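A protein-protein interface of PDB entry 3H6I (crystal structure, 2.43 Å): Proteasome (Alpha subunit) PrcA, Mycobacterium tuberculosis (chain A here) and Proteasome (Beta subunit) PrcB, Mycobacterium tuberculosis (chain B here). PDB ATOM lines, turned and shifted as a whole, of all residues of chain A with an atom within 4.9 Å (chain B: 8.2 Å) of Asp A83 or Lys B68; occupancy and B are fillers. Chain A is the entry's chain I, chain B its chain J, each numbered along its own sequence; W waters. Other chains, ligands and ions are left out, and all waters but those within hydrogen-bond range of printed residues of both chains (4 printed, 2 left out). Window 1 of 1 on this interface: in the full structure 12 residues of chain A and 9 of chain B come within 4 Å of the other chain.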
ATOM      1  N   SER A  54       2.775  17.700 -26.746  1.00  0.00           N
ATOM      2  CA  SER A  54       1.675  18.218 -25.936  1.00  0.00           C
ATOM      3  C   SER A  54       2.045  18.722 -24.560  1.00  0.00           C
ATOM      4  O   SER A  54       3.082  18.349 -24.008  1.00  0.00           O
ATOM      5  CB  SER A  54       0.629  17.124 -25.767  1.00  0.00           C
ATOM      6  OG  SER A  54      -0.510  17.522 -25.004  1.00  0.00           O
ATOM      7  N   GLU A  55       1.194  19.619 -24.050  1.00  0.00           N
ATOM      8  CA  GLU A  55       1.269  20.131 -22.685  1.00  0.00           C
ATOM      9  C   GLU A  55       0.834  18.987 -21.756  1.00  0.00           C
ATOM     10  O   GLU A  55       0.055  18.120 -22.179  1.00  0.00           O
ATOM     11  CB  GLU A  55       0.253  21.251 -22.519  1.00  0.00           C
ATOM     12  CG  GLU A  55       0.285  21.953 -21.147  1.00  0.00           C
ATOM     13  CD  GLU A  55      -0.640  23.160 -21.076  1.00  0.00           C
ATOM     14  OE1 GLU A  55      -1.359  23.432 -22.081  1.00  0.00           O
ATOM     15  OE2 GLU A  55      -0.664  23.820 -19.999  1.00  0.00           O
ATOM     16  N   LEU A  56       1.478  18.861 -20.594  1.00  0.00           N
ATOM     17  CA  LEU A  56       1.047  17.874 -19.602  1.00  0.00           C
ATOM     18  C   LEU A  56       0.538  18.669 -18.397  1.00  0.00           C
ATOM     19  O   LEU A  56      -0.582  18.510 -17.987  1.00  0.00           O
ATOM     20  CB  LEU A  56       2.159  16.950 -19.168  1.00  0.00           C
ATOM     21  CG  LEU A  56       2.545  15.827 -20.124  1.00  0.00           C
ATOM     22  CD1 LEU A  56       3.692  15.021 -19.536  1.00  0.00           C
ATOM     23  CD2 LEU A  56       1.347  14.911 -20.464  1.00  0.00           C
ATOM     24  N   TYR A  57       1.376  19.565 -17.888  1.00  0.00           N
ATOM     25  CA  TYR A  57       1.084  20.391 -16.721  1.00  0.00           C
ATOM     26  C   TYR A  57       1.728  21.767 -16.870  1.00  0.00           C
ATOM     27  O   TYR A  57       2.139  22.128 -17.950  1.00  0.00           O
ATOM     28  CB  TYR A  57       1.512  19.708 -15.430  1.00  0.00           C
ATOM     29  CG  TYR A  57       0.622  20.016 -14.246  1.00  0.00           C
ATOM     30  CD1 TYR A  57      -0.685  19.572 -14.204  1.00  0.00           C
ATOM     31  CD2 TYR A  57       1.095  20.734 -13.167  1.00  0.00           C
ATOM     32  CE1 TYR A  57      -1.488  19.841 -13.135  1.00  0.00           C
ATOM     33  CE2 TYR A  57       0.294  21.006 -12.099  1.00  0.00           C
ATOM     34  CZ  TYR A  57      -0.995  20.554 -12.085  1.00  0.00           C
ATOM     35  OH  TYR A  57      -1.793  20.828 -11.016  1.00  0.00           O
ATOM     36  N   ARG A  75      -0.494   9.993 -23.320  1.00  0.00           N
ATOM     37  CA  ARG A  75      -0.543  11.457 -23.177  1.00  0.00           C
ATOM     38  C   ARG A  75      -1.766  11.812 -22.310  1.00  0.00           C
ATOM     39  O   ARG A  75      -1.652  12.601 -21.362  1.00  0.00           O
ATOM     40  CB  ARG A  75      -0.680  12.119 -24.563  1.00  0.00           C
ATOM     41  CG  ARG A  75      -0.654  13.631 -24.585  1.00  0.00           C
ATOM     42  CD  ARG A  75      -1.065  14.141 -25.969  1.00  0.00           C
ATOM     43  NE  ARG A  75      -2.448  13.876 -26.293  1.00  0.00           N
ATOM     44  CZ  ARG A  75      -3.457  14.689 -26.020  1.00  0.00           C
ATOM     45  NH1 ARG A  75      -3.245  15.860 -25.405  1.00  0.00           N
ATOM     46  NH2 ARG A  75      -4.681  14.298 -26.348  1.00  0.00           N
ATOM     47  N   ILE A  79      -1.987  13.281 -18.419  1.00  0.00           N
ATOM     48  CA  ILE A  79      -2.727  14.501 -18.094  1.00  0.00           C
ATOM     49  C   ILE A  79      -3.685  14.185 -16.925  1.00  0.00           C
ATOM     50  O   ILE A  79      -3.749  14.952 -15.971  1.00  0.00           O
ATOM     51  CB  ILE A  79      -3.464  15.080 -19.326  1.00  0.00           C
ATOM     52  CG1 ILE A  79      -2.443  15.687 -20.290  1.00  0.00           C
ATOM     53  CG2 ILE A  79      -4.455  16.160 -18.907  1.00  0.00           C
ATOM     54  CD1 ILE A  79      -2.982  16.012 -21.680  1.00  0.00           C
ATOM     55  N   GLN A  80      -4.289  12.991 -16.963  1.00  0.00           N
ATOM     56  CA  GLN A  80      -5.195  12.503 -15.918  1.00  0.00           C
ATOM     57  C   GLN A  80      -4.432  12.370 -14.588  1.00  0.00           C
ATOM     58  O   GLN A  80      -4.848  12.881 -13.572  1.00  0.00           O
ATOM     59  CB  GLN A  80      -5.835  11.168 -16.345  1.00  0.00           C
ATOM     60  CG  GLN A  80      -6.895  10.594 -15.416  1.00  0.00           C
ATOM     61  CD  GLN A  80      -8.111  11.508 -15.286  1.00  0.00           C
ATOM     62  OE1 GLN A  80      -8.721  11.910 -16.291  1.00  0.00           O
ATOM     63  NE2 GLN A  80      -8.451  11.863 -14.050  1.00  0.00           N
ATOM     64  N   PHE A  81      -3.245  11.801 -14.647  1.00  0.00           N
ATOM     65  CA  PHE A  81      -2.417  11.653 -13.472  1.00  0.00           C
ATOM     66  C   PHE A  81      -1.994  13.024 -12.885  1.00  0.00           C
ATOM     67  O   PHE A  81      -2.103  13.247 -11.695  1.00  0.00           O
ATOM     68  CB  PHE A  81      -1.175  10.810 -13.821  1.00  0.00           C
ATOM     69  CG  PHE A  81      -0.201  10.647 -12.679  1.00  0.00           C
ATOM     70  CD1 PHE A  81      -0.425   9.673 -11.693  1.00  0.00           C
ATOM     71  CD2 PHE A  81       0.871  11.540 -12.521  1.00  0.00           C
ATOM     72  CE1 PHE A  81       0.397   9.600 -10.551  1.00  0.00           C
ATOM     73  CE2 PHE A  81       1.709  11.478 -11.374  1.00  0.00           C
ATOM     74  CZ  PHE A  81       1.470  10.515 -10.393  1.00  0.00           C
ATOM     75  N   ALA A  82      -1.513  13.915 -13.734  1.00  0.00           N
ATOM     76  CA  ALA A  82      -1.032  15.223 -13.311  1.00  0.00           C
ATOM     77  C   ALA A  82      -2.115  16.102 -12.681  1.00  0.00           C
ATOM     78  O   ALA A  82      -1.886  16.707 -11.642  1.00  0.00           O
ATOM     79  CB  ALA A  82      -0.366  15.927 -14.475  1.00  0.00           C
ATOM     80  N   ASP A  83      -3.295  16.138 -13.305  1.00  0.00           N
ATOM     81  CA  ASP A  83      -4.428  16.908 -12.800  1.00  0.00           C
ATOM     82  C   ASP A  83      -4.959  16.389 -11.466  1.00  0.00           C
ATOM     83  O   ASP A  83      -5.195  17.175 -10.569  1.00  0.00           O
ATOM     84  CB  ASP A  83      -5.517  17.024 -13.845  1.00  0.00           C
ATOM     85  CG  ASP A  83      -5.136  18.002 -14.983  1.00  0.00           C
ATOM     86  OD1 ASP A  83      -4.074  18.665 -14.886  1.00  0.00           O
ATOM     87  OD2 ASP A  83      -5.893  18.117 -15.974  1.00  0.00           O
ATOM     88  N   THR A  84      -4.963  15.066 -11.297  1.00  0.00           N
ATOM     89  CA  THR A  84      -5.381  14.413 -10.053  1.00  0.00           C
ATOM     90  C   THR A  84      -4.366  14.702  -8.935  1.00  0.00           C
ATOM     91  O   THR A  84      -4.757  15.149  -7.859  1.00  0.00           O
ATOM     92  CB  THR A  84      -5.594  12.888 -10.277  1.00  0.00           C
ATOM     93  OG1 THR A  84      -6.706  12.710 -11.167  1.00  0.00           O
ATOM     94  CG2 THR A  84      -5.907  12.132  -8.976  1.00  0.00           C
ATOM     95  N   ARG A  85      -3.074  14.620  -9.241  1.00  0.00           N
ATOM     96  CA  ARG A  85      -2.015  14.892  -8.247  1.00  0.00           C
ATOM     97  C   ARG A  85      -1.971  16.319  -7.781  1.00  0.00           C
ATOM     98  O   ARG A  85      -1.915  16.587  -6.580  1.00  0.00           O
ATOM     99  CB  ARG A  85      -0.625  14.563  -8.789  1.00  0.00           C
ATOM    100  CG  ARG A  85      -0.334  13.108  -8.864  1.00  0.00           C
ATOM    101  CD  ARG A  85      -0.207  12.443  -7.496  1.00  0.00           C
ATOM    102  NE  ARG A  85       0.903  12.992  -6.740  1.00  0.00           N
ATOM    103  CZ  ARG A  85       1.549  12.339  -5.776  1.00  0.00           C
ATOM    104  NH1 ARG A  85       1.192  11.110  -5.448  1.00  0.00           N
ATOM    105  NH2 ARG A  85       2.549  12.922  -5.121  1.00  0.00           N
ATOM    106  N   GLY A  86      -2.050  17.236  -8.736  1.00  0.00           N
ATOM    107  CA  GLY A  86      -2.003  18.645  -8.402  1.00  0.00           C
ATOM    108  C   GLY A  86      -3.188  19.097  -7.582  1.00  0.00           C
ATOM    109  O   GLY A  86      -3.047  19.997  -6.754  1.00  0.00           O
ATOM    110  N   TYR A  87      -4.343  18.461  -7.806  1.00  0.00           N
ATOM    111  CA  TYR A  87      -5.552  18.794  -7.076  1.00  0.00           C
ATOM    112  C   TYR A  87      -5.477  18.257  -5.619  1.00  0.00           C
ATOM    113  O   TYR A  87      -5.816  18.962  -4.687  1.00  0.00           O
ATOM    114  CB  TYR A  87      -6.807  18.252  -7.811  1.00  0.00           C
ATOM    115  CG  TYR A  87      -8.081  18.666  -7.153  1.00  0.00           C
ATOM    116  CD1 TYR A  87      -8.490  20.018  -7.137  1.00  0.00           C
ATOM    117  CD2 TYR A  87      -8.892  17.715  -6.509  1.00  0.00           C
ATOM    118  CE1 TYR A  87      -9.686  20.406  -6.485  1.00  0.00           C
ATOM    119  CE2 TYR A  87     -10.088  18.099  -5.848  1.00  0.00           C
ATOM    120  CZ  TYR A  87     -10.474  19.434  -5.833  1.00  0.00           C
ATOM    121  OH  TYR A  87     -11.602  19.799  -5.133  1.00  0.00           O
ATOM    122  N   ARG A 220       1.617  28.689 -17.453  1.00  0.00           N
ATOM    123  CA  ARG A 220       1.598  27.665 -18.470  1.00  0.00           C
ATOM    124  C   ARG A 220       2.715  27.916 -19.453  1.00  0.00           C
ATOM    125  O   ARG A 220       2.644  28.804 -20.294  1.00  0.00           O
ATOM    126  CB  ARG A 220       0.242  27.642 -19.167  1.00  0.00           C
ATOM    127  CG  ARG A 220      -0.845  27.028 -18.320  1.00  0.00           C
ATOM    128  CD  ARG A 220      -2.203  27.176 -18.947  1.00  0.00           C
ATOM    129  NE  ARG A 220      -2.516  26.103 -19.870  1.00  0.00           N
ATOM    130  CZ  ARG A 220      -3.562  26.119 -20.679  1.00  0.00           C
ATOM    131  NH1 ARG A 220      -4.384  27.151 -20.669  1.00  0.00           N
ATOM    132  NH2 ARG A 220      -3.780  25.107 -21.494  1.00  0.00           N
ATOM    133  N   ARG B  57     -11.477  26.282  -7.824  1.00  0.00           N
ATOM    134  CA  ARG B  57     -10.296  25.472  -8.125  1.00  0.00           C
ATOM    135  C   ARG B  57     -10.639  24.198  -8.894  1.00  0.00           C
ATOM    136  O   ARG B  57      -9.990  23.879  -9.906  1.00  0.00           O
ATOM    137  CB  ARG B  57      -9.491  25.112  -6.871  1.00  0.00           C
ATOM    138  CG  ARG B  57      -8.059  24.505  -7.161  1.00  0.00           C
ATOM    139  CD  ARG B  57      -7.158  24.460  -5.882  1.00  0.00           C
ATOM    140  NE  ARG B  57      -7.725  23.631  -4.812  1.00  0.00           N
ATOM    141  CZ  ARG B  57      -7.272  22.423  -4.434  1.00  0.00           C
ATOM    142  NH1 ARG B  57      -6.210  21.860  -5.013  1.00  0.00           N
ATOM    143  NH2 ARG B  57      -7.943  21.730  -3.517  1.00  0.00           N
ATOM    144  N   LEU B  58     -11.684  23.501  -8.442  1.00  0.00           N
ATOM    145  CA  LEU B  58     -12.088  22.281  -9.102  1.00  0.00           C
ATOM    146  C   LEU B  58     -12.602  22.593 -10.504  1.00  0.00           C
ATOM    147  O   LEU B  58     -12.283  21.881 -11.441  1.00  0.00           O
ATOM    148  CB  LEU B  58     -13.156  21.541  -8.285  1.00  0.00           C
ATOM    149  CG  LEU B  58     -13.572  20.167  -8.828  1.00  0.00           C
ATOM    150  CD1 LEU B  58     -12.343  19.231  -9.099  1.00  0.00           C
ATOM    151  CD2 LEU B  58     -14.517  19.518  -7.838  1.00  0.00           C
ATOM    152  N   ALA B  60     -11.767  25.213 -12.426  1.00  0.00           N
ATOM    153  CA  ALA B  60     -10.657  25.659 -13.268  1.00  0.00           C
ATOM    154  C   ALA B  60      -9.823  24.466 -13.728  1.00  0.00           C
ATOM    155  O   ALA B  60      -9.444  24.406 -14.886  1.00  0.00           O
ATOM    156  CB  ALA B  60      -9.802  26.687 -12.575  1.00  0.00           C
ATOM    157  N   VAL B  61      -9.670  23.463 -12.860  1.00  0.00           N
ATOM    158  CA  VAL B  61      -8.938  22.261 -13.209  1.00  0.00           C
ATOM    159  C   VAL B  61      -9.735  21.507 -14.299  1.00  0.00           C
ATOM    160  O   VAL B  61      -9.153  21.082 -15.283  1.00  0.00           O
ATOM    161  CB  VAL B  61      -8.663  21.379 -11.980  1.00  0.00           C
ATOM    162  CG1 VAL B  61      -8.155  19.973 -12.369  1.00  0.00           C
ATOM    163  CG2 VAL B  61      -7.624  22.047 -11.124  1.00  0.00           C
ATOM    164  N   GLU B  62     -11.062  21.459 -14.179  1.00  0.00           N
ATOM    165  CA  GLU B  62     -11.866  20.774 -15.177  1.00  0.00           C
ATOM    166  C   GLU B  62     -11.805  21.444 -16.562  1.00  0.00           C
ATOM    167  O   GLU B  62     -11.596  20.755 -17.562  1.00  0.00           O
ATOM    168  CB  GLU B  62     -13.306  20.560 -14.701  1.00  0.00           C
ATOM    169  CG  GLU B  62     -14.205  19.840 -15.722  1.00  0.00           C
ATOM    170  CD  GLU B  62     -14.945  18.667 -15.154  1.00  0.00           C
ATOM    171  OE1 GLU B  62     -14.279  17.676 -14.782  1.00  0.00           O
ATOM    172  OE2 GLU B  62     -16.197  18.737 -15.087  1.00  0.00           O
ATOM    173  N   LEU B  63     -11.857  22.773 -16.618  1.00  0.00           N
ATOM    174  CA  LEU B  63     -11.774  23.450 -17.910  1.00  0.00           C
ATOM    175  C   LEU B  63     -10.415  23.284 -18.601  1.00  0.00           C
ATOM    176  O   LEU B  63     -10.355  23.030 -19.832  1.00  0.00           O
ATOM    177  CB  LEU B  63     -12.077  24.927 -17.769  1.00  0.00           C
ATOM    178  CG  LEU B  63     -13.475  25.289 -17.285  1.00  0.00           C
ATOM    179  CD1 LEU B  63     -13.600  26.763 -17.120  1.00  0.00           C
ATOM    180  CD2 LEU B  63     -14.550  24.759 -18.226  1.00  0.00           C
ATOM    181  N   GLU B  64      -9.333  23.342 -17.805  1.00  0.00           N
ATOM    182  CA  GLU B  64      -7.991  23.198 -18.359  1.00  0.00           C
ATOM    183  C   GLU B  64      -7.683  21.760 -18.706  1.00  0.00           C
ATOM    184  O   GLU B  64      -6.940  21.494 -19.636  1.00  0.00           O
ATOM    185  CB  GLU B  64      -6.925  23.743 -17.441  1.00  0.00           C
ATOM    186  CG  GLU B  64      -5.544  23.956 -18.105  1.00  0.00           C
ATOM    187  CD  GLU B  64      -4.645  24.871 -17.272  1.00  0.00           C
ATOM    188  OE1 GLU B  64      -4.871  26.109 -17.325  1.00  0.00           O
ATOM    189  OE2 GLU B  64      -3.747  24.362 -16.550  1.00  0.00           O
ATOM    190  N   HIS B  65      -8.343  20.843 -18.013  1.00  0.00           N
ATOM    191  CA  HIS B  65      -8.152  19.406 -18.224  1.00  0.00           C
ATOM    192  C   HIS B  65      -8.696  19.067 -19.620  1.00  0.00           C
ATOM    193  O   HIS B  65      -8.013  18.406 -20.413  1.00  0.00           O
ATOM    194  CB  HIS B  65      -8.889  18.658 -17.124  1.00  0.00           C
ATOM    195  CG  HIS B  65      -8.799  17.177 -17.207  1.00  0.00           C
ATOM    196  ND1 HIS B  65      -7.680  16.495 -16.810  1.00  0.00           N
ATOM    197  CD2 HIS B  65      -9.719  16.243 -17.555  1.00  0.00           C
ATOM    198  CE1 HIS B  65      -7.910  15.200 -16.897  1.00  0.00           C
ATOM    199  NE2 HIS B  65      -9.136  15.019 -17.348  1.00  0.00           N
ATOM    200  N   TYR B  66      -9.843  19.665 -19.952  1.00  0.00           N
ATOM    201  CA  TYR B  66     -10.429  19.447 -21.247  1.00  0.00           C
ATOM    202  C   TYR B  66      -9.535  20.045 -22.345  1.00  0.00           C
ATOM    203  O   TYR B  66      -9.240  19.362 -23.330  1.00  0.00           O
ATOM    204  CB  TYR B  66     -11.841  20.010 -21.309  1.00  0.00           C
ATOM    205  CG  TYR B  66     -12.499  19.765 -22.651  1.00  0.00           C
ATOM    206  CD1 TYR B  66     -13.311  18.638 -22.844  1.00  0.00           C
ATOM    207  CD2 TYR B  66     -12.299  20.661 -23.746  1.00  0.00           C
ATOM    208  CE1 TYR B  66     -13.918  18.391 -24.087  1.00  0.00           C
ATOM    209  CE2 TYR B  66     -12.874  20.431 -24.966  1.00  0.00           C
ATOM    210  CZ  TYR B  66     -13.692  19.285 -25.132  1.00  0.00           C
ATOM    211  OH  TYR B  66     -14.275  19.041 -26.320  1.00  0.00           O
ATOM    212  N   GLU B  67      -9.121  21.296 -22.166  1.00  0.00           N
ATOM    213  CA  GLU B  67      -8.262  21.973 -23.140  1.00  0.00           C
ATOM    214  C   GLU B  67      -6.954  21.210 -23.450  1.00  0.00           C
ATOM    215  O   GLU B  67      -6.561  21.113 -24.600  1.00  0.00           O
ATOM    216  CB  GLU B  67      -7.950  23.385 -22.663  1.00  0.00           C
ATOM    217  CG  GLU B  67      -7.303  24.266 -23.720  1.00  0.00           C
ATOM    218  CD  GLU B  67      -6.722  25.564 -23.188  1.00  0.00           C
ATOM    219  OE1 GLU B  67      -7.092  26.005 -22.068  1.00  0.00           O
ATOM    220  OE2 GLU B  67      -5.895  26.157 -23.918  1.00  0.00           O
ATOM    221  N   LYS B  68      -6.328  20.617 -22.436  1.00  0.00           N
ATOM    222  CA  LYS B  68      -5.100  19.871 -22.644  1.00  0.00           C
ATOM    223  C   LYS B  68      -5.373  18.544 -23.311  1.00  0.00           C
ATOM    224  O   LYS B  68      -4.573  18.099 -24.114  1.00  0.00           O
ATOM    225  CB  LYS B  68      -4.351  19.644 -21.335  1.00  0.00           C
ATOM    226  CG  LYS B  68      -3.762  20.937 -20.734  1.00  0.00           C
ATOM    227  CD  LYS B  68      -2.972  20.704 -19.456  1.00  0.00           C
ATOM    228  CE  LYS B  68      -3.755  19.987 -18.363  1.00  0.00           C
ATOM    229  NZ  LYS B  68      -2.976  20.009 -17.086  1.00  0.00           N
ATOM    230  N   LEU B  69      -6.501  17.917 -22.978  1.00  0.00           N
ATOM    231  CA  LEU B  69      -6.838  16.642 -23.567  1.00  0.00           C
ATOM    232  C   LEU B  69      -7.267  16.715 -25.015  1.00  0.00           C
ATOM    233  O   LEU B  69      -6.821  15.917 -25.808  1.00  0.00           O
ATOM    234  CB  LEU B  69      -7.929  15.929 -22.788  1.00  0.00           C
ATOM    235  CG  LEU B  69      -7.596  15.252 -21.462  1.00  0.00           C
ATOM    236  CD1 LEU B  69      -8.870  14.660 -20.867  1.00  0.00           C
ATOM    237  CD2 LEU B  69      -6.605  14.184 -21.660  1.00  0.00           C
ATOM    238  N   GLU B  70      -8.101  17.682 -25.359  1.00  0.00           N
ATOM    239  CA  GLU B  70      -8.605  17.794 -26.714  1.00  0.00           C
ATOM    240  C   GLU B  70      -7.978  18.898 -27.554  1.00  0.00           C
ATOM    241  O   GLU B  70      -8.290  19.025 -28.718  1.00  0.00           O
ATOM    242  CB  GLU B  70     -10.118  17.961 -26.699  1.00  0.00           C
ATOM    243  CG  GLU B  70     -10.834  17.077 -25.705  1.00  0.00           C
ATOM    244  CD  GLU B  70     -10.650  15.606 -25.976  1.00  0.00           C
ATOM    245  OE1 GLU B  70     -10.557  15.205 -27.142  1.00  0.00           O
ATOM    246  OE2 GLU B  70     -10.603  14.841 -25.014  1.00  0.00           O
ATOM    247  N   GLY B  71      -7.097  19.697 -26.976  1.00  0.00           N
ATOM    248  CA  GLY B  71      -6.416  20.715 -27.762  1.00  0.00           C
ATOM    249  C   GLY B  71      -7.131  22.038 -27.950  1.00  0.00           C
ATOM    250  O   GLY B  71      -6.523  23.004 -28.417  1.00  0.00           O
ATOM    251  N   VAL B  72      -8.391  22.115 -27.555  1.00  0.00           N
ATOM    252  CA  VAL B  72      -9.156  23.354 -27.751  1.00  0.00           C
ATOM    253  C   VAL B  72     -10.057  23.532 -26.512  1.00  0.00           C
ATOM    254  O   VAL B  72     -10.290  22.548 -25.817  1.00  0.00           O
ATOM    255  CB  VAL B  72      -9.977  23.196 -29.104  1.00  0.00           C
ATOM    256  CG1 VAL B  72     -11.133  22.222 -28.961  1.00  0.00           C
ATOM    257  CG2 VAL B  72     -10.424  24.528 -29.662  1.00  0.00           C
ATOM    258  N   PRO B  73     -10.438  24.784 -26.129  1.00  0.00           N
ATOM    259  CA  PRO B  73     -11.325  24.908 -24.947  1.00  0.00           C
ATOM    260  C   PRO B  73     -12.743  24.434 -25.300  1.00  0.00           C
ATOM    261  O   PRO B  73     -13.138  24.425 -26.480  1.00  0.00           O
ATOM    262  CB  PRO B  73     -11.423  26.433 -24.735  1.00  0.00           C
ATOM    263  CG  PRO B  73     -10.213  26.967 -25.377  1.00  0.00           C
ATOM    264  CD  PRO B  73      -9.990  26.122 -26.576  1.00  0.00           C
HETATM  265  O   HOH W   1      -4.022  22.376  -6.140  1.00  0.00           O
HETATM  266  O   HOH W   2     -10.587  12.595 -18.269  1.00  0.00           O
HETATM  267  O   HOH W   3      -6.134  20.877 -15.881  1.00  0.00           O
HETATM  268  O   HOH W   4      -1.402  23.049 -17.401  1.00  0.00           O
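Hydrophobic or aromatic side chains of chain A that line the printed part of chain B: Tyr A57, Ile A79 and Tyr A87.
Along chain A the printed residues that touch a printed residue of chain B span positions 55 to 220.
Among the printed residues, 14 pairs touch across the chains.
The side-chain hydroxyl (OG) of Ser A54 sits at hydrogen-bond distance from the guanidinium group (NH1) of Arg A75.
The guanidinium group of Arg A220 lies within salt-bridge range of the side-chain carboxylate of Glu A55.
The side-chain hydroxyl (OG1) of Thr A84 is in hydrogen-bond range of the backbone carbonyl oxygen (O) of Gln A80, 3.0 Å away.
Among the printed residues, merely in contact across the chains: Glu A55 with Lys B68 (3.7 Å), Tyr A57 with Lys B68 (3.7 Å), Ile A79 with His B65 (3.9 Å), Ile A79 with Lys B68 (3.6 Å) and Tyr A87 with Leu B58 (3.8 Å).
Asp A83 touches just these residues of chain B: His B65 and Lys B68.
Lys B68 touches just these residues of chain A: Glu A55, Leu A56, Tyr A57, Arg A75, Ile A79 and Asp A83.
No residue of chain B comes within 4 Å of Ala A82.
Of the printed residues of chain A, Glu B67 touches Arg A220.
Printed residues of chain A within 4 Å of Glu B64: Arg A220 (3.3 Å).
The nearest printed residue of chain B that does not touch Glu A55 is Glu B64 (4.7 Å).
The backbone carbonyl oxygen (O) of Leu A56 sits at hydrogen-bond distance from the side-chain amino group (NZ) of Lys B68 (3.0 Å).
The guanidinium group of Arg A75 is in hydrogen-bond range of the backbone carbonyl oxygen of Lys B68 (2.9 Å).
The guanidinium group (NH2) of Arg A75 lies within hydrogen-bond range of the backbone carbonyl oxygen (O) of Leu B69 (2.7 Å).
A ring nitrogen (NE2) of His B65 is in hydrogen-bond range of the side-chain amide oxygen (OE1) of Gln A80, at 3.3 Å.
ND1 of His B65 sits at hydrogen-bond distance from OD2 of Asp A83, at 2.6 Å.
The side-chain carboxylate of Asp A83 lies within salt-bridge range of the side-chain amino group of Lys B68 (2.8 Å).
O of Tyr A87 sits at hydrogen-bond distance from NH1 of Arg B57 (2.9 Å).
The guanidinium group (NE) of Arg A220 lies within salt-bridge range of the side-chain carboxylate (OE1) of Glu B64 (3.5 Å).
The guanidinium group (NH1) of Arg A220 lies within salt-bridge range of the side-chain carboxylate (OE1) of Glu B67, at 3.3 Å.
Water W1 bridges the guanidinium group of Arg B57 and the backbone carbonyl oxygen of Gly A86.
Water W3 lies within hydrogen-bond range of the side-chain carboxylate of Asp A83 (2.8 Å), the backbone NH of His B65 (3.1 Å), the backbone carbonyl oxygen of Val B61 (3.1 Å) and the side-chain amino group of Lys B68 (3.5 Å).
Water W2 lies within hydrogen-bond range of the side-chain amide oxygen of Gln A80 and a ring nitrogen (NE2) of His B65.
Water W4 lies within hydrogen-bond range of the side-chain carboxylate of Glu A55, the side-chain carboxylate of Glu B64 and the side-chain amino group of Lys B68.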
